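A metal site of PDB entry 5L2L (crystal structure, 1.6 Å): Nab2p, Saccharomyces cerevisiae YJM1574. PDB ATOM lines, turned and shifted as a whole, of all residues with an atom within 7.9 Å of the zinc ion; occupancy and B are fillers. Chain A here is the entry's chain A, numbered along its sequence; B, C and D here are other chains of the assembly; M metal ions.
A ring nitrogen (ND1) of His 24 lies close to the backbone carbonyl oxygen (O) of Tyr 22 (3.0 Å). N of Phe 11 sits close to SG of Cys 9 (3.5 Å). The backbone carbonyl oxygen (O) of Arg 23 sits at hydrogen-bond distance from the backbone NH (N) of Cys 9 (2.8 Å). SG of Cys 20 sits close to N of Tyr 22, 3.6 Å away. SG of Cys 15 sits close to N6 of A 4 of chain C. The side-chain sulfur (SG) of Cys 15 sits close to the backbone NH (N) of Asn 17, 3.6 Å away. The backbone carbonyl oxygen (O) of Cys 15 is in hydrogen-bond range of the side-chain amino group (NZ) of Lys 18 of chain D (2.7 Å).
Within 4 Å of the zinc ion: Cys 9, Cys 15, Cys 20 and His 24.
The zinc ion is bound by NE2 of His 24 (2.1 Å), SG of Cys 9 (2.3 Å), SG of Cys 20 (2.4 Å) and SG of Cys 15 (2.4 Å). The zinc ion has four donor atoms within binding distance.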
ATOM      1  N   GLU A   7      12.252 -26.073  16.748  1.00  0.00           N
ATOM      2  CA  GLU A   7      13.373 -25.241  16.350  1.00  0.00           C
ATOM      3  C   GLU A   7      13.370 -23.918  17.132  1.00  0.00           C
ATOM      4  O   GLU A   7      12.311 -23.339  17.393  1.00  0.00           O
ATOM      5  CB  GLU A   7      13.309 -25.028  14.817  1.00  0.00           C
ATOM      6  CG  GLU A   7      14.317 -24.040  14.239  1.00  0.00           C
ATOM      7  CD  GLU A   7      14.239 -23.879  12.712  1.00  0.00           C
ATOM      8  OE1 GLU A   7      14.626 -22.789  12.199  1.00  0.00           O
ATOM      9  OE2 GLU A   7      13.818 -24.848  12.029  1.00  0.00           O
ATOM     10  N   GLN A   8      14.562 -23.456  17.515  1.00  0.00           N
ATOM     11  CA  GLN A   8      14.715 -22.260  18.347  1.00  0.00           C
ATOM     12  C   GLN A   8      14.587 -20.975  17.526  1.00  0.00           C
ATOM     13  O   GLN A   8      15.237 -20.828  16.479  1.00  0.00           O
ATOM     14  CB  GLN A   8      16.076 -22.286  19.045  1.00  0.00           C
ATOM     15  CG  GLN A   8      16.193 -21.315  20.216  1.00  0.00           C
ATOM     16  CD  GLN A   8      15.360 -21.776  21.402  1.00  0.00           C
ATOM     17  OE1 GLN A   8      15.079 -22.972  21.535  1.00  0.00           O
ATOM     18  NE2 GLN A   8      14.965 -20.859  22.259  1.00  0.00           N
ATOM     19  N   CYS A   9      13.776 -20.022  18.017  1.00  0.00           N
ATOM     20  CA  CYS A   9      13.697 -18.694  17.381  1.00  0.00           C
ATOM     21  C   CYS A   9      14.991 -17.928  17.620  1.00  0.00           C
ATOM     22  O   CYS A   9      15.444 -17.777  18.759  1.00  0.00           O
ATOM     23  CB  CYS A   9      12.517 -17.885  17.931  1.00  0.00           C
ATOM     24  SG  CYS A   9      12.360 -16.238  17.124  1.00  0.00           S
ATOM     25  N   LYS A  10      15.573 -17.398  16.536  1.00  0.00           N
ATOM     26  CA  LYS A  10      16.846 -16.709  16.672  1.00  0.00           C
ATOM     27  C   LYS A  10      16.710 -15.339  17.327  1.00  0.00           C
ATOM     28  O   LYS A  10      17.746 -14.754  17.713  1.00  0.00           O
ATOM     29  CB  LYS A  10      17.562 -16.589  15.314  1.00  0.00           C
ATOM     30  CG  LYS A  10      16.842 -15.811  14.272  1.00  0.00           C
ATOM     31  CD  LYS A  10      17.589 -15.893  12.901  1.00  0.00           C
ATOM     32  CE  LYS A  10      18.989 -15.320  13.007  1.00  0.00           C
ATOM     33  NZ  LYS A  10      19.676 -15.105  11.665  1.00  0.00           N
ATOM     34  N   PHE A  11      15.493 -14.821  17.505  1.00  0.00           N
ATOM     35  CA  PHE A  11      15.287 -13.479  18.069  1.00  0.00           C
ATOM     36  C   PHE A  11      14.868 -13.485  19.540  1.00  0.00           C
ATOM     37  O   PHE A  11      14.851 -12.419  20.170  1.00  0.00           O
ATOM     38  CB  PHE A  11      14.268 -12.706  17.219  1.00  0.00           C
ATOM     39  CG  PHE A  11      14.594 -12.705  15.743  1.00  0.00           C
ATOM     40  CD1 PHE A  11      15.698 -12.038  15.261  1.00  0.00           C
ATOM     41  CD2 PHE A  11      13.804 -13.412  14.853  1.00  0.00           C
ATOM     42  CE1 PHE A  11      16.020 -12.058  13.909  1.00  0.00           C
ATOM     43  CE2 PHE A  11      14.107 -13.442  13.495  1.00  0.00           C
ATOM     44  CZ  PHE A  11      15.212 -12.755  13.027  1.00  0.00           C
ATOM     45  N   GLY A  12      14.509 -14.642  20.103  1.00  0.00           N
ATOM     46  CA  GLY A  12      14.245 -14.730  21.535  1.00  0.00           C
ATOM     47  C   GLY A  12      13.147 -13.786  22.013  1.00  0.00           C
ATOM     48  O   GLY A  12      12.086 -13.671  21.388  1.00  0.00           O
ATOM     49  N   THR A  13      13.389 -13.101  23.133  1.00  0.00           N
ATOM     50  CA  THR A  13      12.378 -12.199  23.699  1.00  0.00           C
ATOM     51  C   THR A  13      12.172 -10.950  22.851  1.00  0.00           C
ATOM     52  O   THR A  13      11.237 -10.181  23.117  1.00  0.00           O
ATOM     53  CB  THR A  13      12.752 -11.792  25.135  1.00  0.00           C
ATOM     54  OG1 THR A  13      14.034 -11.158  25.143  1.00  0.00           O
ATOM     55  CG2 THR A  13      12.769 -12.973  26.102  1.00  0.00           C
ATOM     56  N   HIS A  14      13.001 -10.724  21.824  1.00  0.00           N
ATOM     57  CA  HIS A  14      12.841  -9.566  20.954  1.00  0.00           C
ATOM     58  C   HIS A  14      12.232  -9.922  19.600  1.00  0.00           C
ATOM     59  O   HIS A  14      12.218  -9.077  18.687  1.00  0.00           O
ATOM     60  CB  HIS A  14      14.199  -8.894  20.786  1.00  0.00           C
ATOM     61  CG  HIS A  14      14.943  -8.836  22.077  1.00  0.00           C
ATOM     62  ND1 HIS A  14      14.534  -8.053  23.134  1.00  0.00           N
ATOM     63  CD2 HIS A  14      16.019  -9.531  22.517  1.00  0.00           C
ATOM     64  CE1 HIS A  14      15.340  -8.244  24.168  1.00  0.00           C
ATOM     65  NE2 HIS A  14      16.249  -9.141  23.812  1.00  0.00           N
ATOM     66  N   CYS A  15      11.680 -11.132  19.477  1.00  0.00           N
ATOM     67  CA  CYS A  15      10.885 -11.499  18.313  1.00  0.00           C
ATOM     68  C   CYS A  15       9.591 -10.694  18.270  1.00  0.00           C
ATOM     69  O   CYS A  15       8.882 -10.585  19.278  1.00  0.00           O
ATOM     70  CB  CYS A  15      10.566 -12.986  18.367  1.00  0.00           C
ATOM     71  SG  CYS A  15       9.576 -13.596  16.960  1.00  0.00           S
ATOM     72  N   THR A  16       9.277 -10.139  17.091  1.00  0.00           N
ATOM     73  CA  THR A  16       8.064  -9.345  16.936  1.00  0.00           C
ATOM     74  C   THR A  16       7.142  -9.903  15.843  1.00  0.00           C
ATOM     75  O   THR A  16       6.221  -9.200  15.392  1.00  0.00           O
ATOM     76  CB  THR A  16       8.406  -7.875  16.683  1.00  0.00           C
ATOM     77  OG1 THR A  16       9.194  -7.729  15.495  1.00  0.00           O
ATOM     78  CG2 THR A  16       9.184  -7.326  17.873  1.00  0.00           C
ATOM     79  N   ASN A  17       7.342 -11.166  15.451  1.00  0.00           N
ATOM     80  CA  ASN A  17       6.436 -11.898  14.571  1.00  0.00           C
ATOM     81  C   ASN A  17       5.313 -12.522  15.401  1.00  0.00           C
ATOM     82  O   ASN A  17       5.520 -13.522  16.091  1.00  0.00           O
ATOM     83  CB  ASN A  17       7.202 -12.983  13.809  1.00  0.00           C
ATOM     84  CG  ASN A  17       6.319 -13.822  12.887  1.00  0.00           C
ATOM     85  OD1 ASN A  17       5.125 -13.568  12.762  1.00  0.00           O
ATOM     86  ND2 ASN A  17       6.923 -14.809  12.207  1.00  0.00           N
ATOM     87  N   LYS A  18       4.096 -11.950  15.301  1.00  0.00           N
ATOM     88  CA  LYS A  18       2.988 -12.407  16.133  1.00  0.00           C
ATOM     89  C   LYS A  18       2.481 -13.797  15.756  1.00  0.00           C
ATOM     90  O   LYS A  18       1.710 -14.394  16.524  1.00  0.00           O
ATOM     91  CB  LYS A  18       1.844 -11.395  16.037  1.00  0.00           C
ATOM     92  CG  LYS A  18       2.202  -9.971  16.500  1.00  0.00           C
ATOM     93  CD  LYS A  18       2.105  -9.808  18.007  1.00  0.00           C
ATOM     94  CE  LYS A  18       1.528  -8.439  18.400  1.00  0.00           C
ATOM     95  NZ  LYS A  18       2.328  -7.287  17.842  1.00  0.00           N
ATOM     96  N   ARG A  19       2.904 -14.345  14.610  1.00  0.00           N
ATOM     97  CA  ARG A  19       2.568 -15.726  14.234  1.00  0.00           C
ATOM     98  C   ARG A  19       3.776 -16.655  14.304  1.00  0.00           C
ATOM     99  O   ARG A  19       3.741 -17.740  13.712  1.00  0.00           O
ATOM    100  CB  ARG A  19       1.962 -15.753  12.837  1.00  0.00           C
ATOM    101  CG  ARG A  19       0.593 -15.068  12.751  1.00  0.00           C
ATOM    102  CD  ARG A  19      -0.140 -15.458  11.485  1.00  0.00           C
ATOM    103  NE  ARG A  19      -1.370 -14.683  11.287  1.00  0.00           N
ATOM    104  CZ  ARG A  19      -2.588 -15.073  11.668  1.00  0.00           C
ATOM    105  NH1 ARG A  19      -2.786 -16.235  12.282  1.00  0.00           N
ATOM    106  NH2 ARG A  19      -3.625 -14.288  11.424  1.00  0.00           N
ATOM    107  N   CYS A  20       4.842 -16.259  14.988  1.00  0.00           N
ATOM    108  CA  CYS A  20       6.044 -17.086  15.041  1.00  0.00           C
ATOM    109  C   CYS A  20       5.750 -18.477  15.599  1.00  0.00           C
ATOM    110  O   CYS A  20       5.132 -18.622  16.670  1.00  0.00           O
ATOM    111  CB  CYS A  20       7.125 -16.391  15.888  1.00  0.00           C
ATOM    112  SG  CYS A  20       8.737 -17.242  15.768  1.00  0.00           S
ATOM    113  N   LYS A  21       6.223 -19.501  14.898  1.00  0.00           N
ATOM    114  CA  LYS A  21       5.969 -20.871  15.314  1.00  0.00           C
ATOM    115  C   LYS A  21       7.107 -21.513  16.109  1.00  0.00           C
ATOM    116  O   LYS A  21       7.000 -22.682  16.461  1.00  0.00           O
ATOM    117  CB  LYS A  21       5.663 -21.739  14.091  1.00  0.00           C
ATOM    118  CG  LYS A  21       6.830 -21.990  13.176  1.00  0.00           C
ATOM    119  CD  LYS A  21       6.309 -22.606  11.873  1.00  0.00           C
ATOM    120  CE  LYS A  21       7.420 -23.014  10.946  1.00  0.00           C
ATOM    121  NZ  LYS A  21       6.887 -23.291   9.566  1.00  0.00           N
ATOM    122  N   TYR A  22       8.178 -20.776  16.403  1.00  0.00           N
ATOM    123  CA  TYR A  22       9.388 -21.348  16.991  1.00  0.00           C
ATOM    124  C   TYR A  22       9.433 -21.140  18.520  1.00  0.00           C
ATOM    125  O   TYR A  22       8.588 -20.470  19.112  1.00  0.00           O
ATOM    126  CB  TYR A  22      10.614 -20.745  16.275  1.00  0.00           C
ATOM    127  CG  TYR A  22      10.605 -21.097  14.792  1.00  0.00           C
ATOM    128  CD1 TYR A  22      10.824 -22.405  14.377  1.00  0.00           C
ATOM    129  CD2 TYR A  22      10.314 -20.153  13.810  1.00  0.00           C
ATOM    130  CE1 TYR A  22      10.788 -22.763  13.033  1.00  0.00           C
ATOM    131  CE2 TYR A  22      10.281 -20.500  12.444  1.00  0.00           C
ATOM    132  CZ  TYR A  22      10.517 -21.812  12.075  1.00  0.00           C
ATOM    133  OH  TYR A  22      10.485 -22.199  10.745  1.00  0.00           O
ATOM    134  N   ARG A  23      10.417 -21.786  19.170  1.00  0.00           N
ATOM    135  CA  ARG A  23      10.568 -21.685  20.629  1.00  0.00           C
ATOM    136  C   ARG A  23      11.333 -20.435  21.035  1.00  0.00           C
ATOM    137  O   ARG A  23      12.293 -20.025  20.361  1.00  0.00           O
ATOM    138  CB  ARG A  23      11.256 -22.935  21.185  1.00  0.00           C
ATOM    139  CG  ARG A  23      10.419 -24.204  21.050  1.00  0.00           C
ATOM    140  CD  ARG A  23      10.836 -25.294  22.073  1.00  0.00           C
ATOM    141  NE  ARG A  23      12.044 -25.996  21.681  1.00  0.00           N
ATOM    142  CZ  ARG A  23      12.563 -27.019  22.369  1.00  0.00           C
ATOM    143  NH1 ARG A  23      11.979 -27.444  23.482  1.00  0.00           N
ATOM    144  NH2 ARG A  23      13.679 -27.607  21.944  1.00  0.00           N
ATOM    145  N   HIS A  24      10.921 -19.817  22.143  1.00  0.00           N
ATOM    146  CA  HIS A  24      11.516 -18.562  22.614  1.00  0.00           C
ATOM    147  C   HIS A  24      12.053 -18.727  24.036  1.00  0.00           C
ATOM    148  O   HIS A  24      11.304 -19.103  24.964  1.00  0.00           O
ATOM    149  CB  HIS A  24      10.497 -17.416  22.558  1.00  0.00           C
ATOM    150  CG  HIS A  24       9.964 -17.168  21.175  1.00  0.00           C
ATOM    151  ND1 HIS A  24       8.919 -17.888  20.639  1.00  0.00           N
ATOM    152  CD2 HIS A  24      10.378 -16.315  20.199  1.00  0.00           C
ATOM    153  CE1 HIS A  24       8.683 -17.475  19.415  1.00  0.00           C
ATOM    154  NE2 HIS A  24       9.565 -16.529  19.117  1.00  0.00           N
ATOM    155  P     A B   3       9.120 -20.585   7.698  1.00  0.00           P
ATOM    156  OP1   A B   3       8.102 -21.192   6.792  1.00  0.00           O
ATOM    157  OP2   A B   3      10.545 -20.987   7.516  1.00  0.00           O
ATOM    158  O5'   A B   3       9.048 -18.994   7.530  1.00  0.00           O
ATOM    159  C5'   A B   3       8.125 -18.217   8.290  1.00  0.00           C
ATOM    160  C4'   A B   3       8.801 -17.031   8.945  1.00  0.00           C
ATOM    161  O4'   A B   3       9.640 -17.504  10.040  1.00  0.00           O
ATOM    162  C3'   A B   3       9.704 -16.204   8.029  1.00  0.00           C
ATOM    163  O3'   A B   3       9.628 -14.821   8.394  1.00  0.00           O
ATOM    164  C2'   A B   3      11.092 -16.759   8.369  1.00  0.00           C
ATOM    165  O2'   A B   3      12.147 -15.875   8.058  1.00  0.00           O
ATOM    166  C1'   A B   3      10.951 -17.003   9.864  1.00  0.00           C
ATOM    167  N9    A B   3      11.893 -17.972  10.458  1.00  0.00           N
ATOM    168  C8    A B   3      12.345 -19.166   9.952  1.00  0.00           C
ATOM    169  N7    A B   3      13.162 -19.810  10.765  1.00  0.00           N
ATOM    170  C5    A B   3      13.257 -18.981  11.890  1.00  0.00           C
ATOM    171  C6    A B   3      13.968 -19.071  13.117  1.00  0.00           C
ATOM    172  N6    A B   3      14.767 -20.080  13.468  1.00  0.00           N
ATOM    173  N1    A B   3      13.836 -18.056  13.997  1.00  0.00           N
ATOM    174  C2    A B   3      13.031 -17.031  13.688  1.00  0.00           C
ATOM    175  N3    A B   3      12.328 -16.839  12.578  1.00  0.00           N
ATOM    176  C4    A B   3      12.477 -17.852  11.709  1.00  0.00           C
ATOM    177  P     A C   4      15.912 -11.418   7.329  1.00  0.00           P
ATOM    178  OP1   A C   4      17.297 -11.844   6.998  1.00  0.00           O
ATOM    179  OP2   A C   4      14.852 -12.389   7.636  1.00  0.00           O
ATOM    180  O5'   A C   4      15.981 -10.546   8.674  1.00  0.00           O
ATOM    181  C5'   A C   4      16.629  -9.295   8.680  1.00  0.00           C
ATOM    182  C4'   A C   4      16.311  -8.475   9.898  1.00  0.00           C
ATOM    183  O4'   A C   4      14.879  -8.315  10.059  1.00  0.00           O
ATOM    184  C3'   A C   4      16.791  -8.999  11.255  1.00  0.00           C
ATOM    185  O3'   A C   4      18.145  -8.648  11.491  1.00  0.00           O
ATOM    186  C2'   A C   4      15.859  -8.269  12.219  1.00  0.00           C
ATOM    187  O2'   A C   4      16.320  -6.935  12.409  1.00  0.00           O
ATOM    188  C1'   A C   4      14.551  -8.233  11.429  1.00  0.00           C
ATOM    189  N9    A C   4      13.634  -9.346  11.771  1.00  0.00           N
ATOM    190  C8    A C   4      13.261 -10.411  10.979  1.00  0.00           C
ATOM    191  N7    A C   4      12.414 -11.246  11.545  1.00  0.00           N
ATOM    192  C5    A C   4      12.227 -10.694  12.808  1.00  0.00           C
ATOM    193  C6    A C   4      11.434 -11.104  13.918  1.00  0.00           C
ATOM    194  N6    A C   4      10.682 -12.219  13.911  1.00  0.00           N
ATOM    195  N1    A C   4      11.439 -10.343  15.035  1.00  0.00           N
ATOM    196  C2    A C   4      12.217  -9.237  15.024  1.00  0.00           C
ATOM    197  N3    A C   4      12.995  -8.730  14.047  1.00  0.00           N
ATOM    198  C4    A C   4      12.961  -9.526  12.954  1.00  0.00           C
ATOM    199  N   LYS D  18       5.181  -7.508  25.328  1.00  0.00           N
ATOM    200  CA  LYS D  18       4.623  -8.855  25.444  1.00  0.00           C
ATOM    201  C   LYS D  18       3.627  -8.982  26.594  1.00  0.00           C
ATOM    202  O   LYS D  18       2.839  -9.926  26.624  1.00  0.00           O
ATOM    203  CB  LYS D  18       5.755  -9.874  25.643  1.00  0.00           C
ATOM    204  CG  LYS D  18       6.828  -9.865  24.550  1.00  0.00           C
ATOM    205  CD  LYS D  18       6.337 -10.585  23.315  1.00  0.00           C
ATOM    206  CE  LYS D  18       7.470 -11.341  22.621  1.00  0.00           C
ATOM    207  NZ  LYS D  18       8.452 -10.428  21.982  1.00  0.00           N
HETATM  208 ZN    ZN M   1      10.064 -15.896  17.167  1.00  0.00          ZN
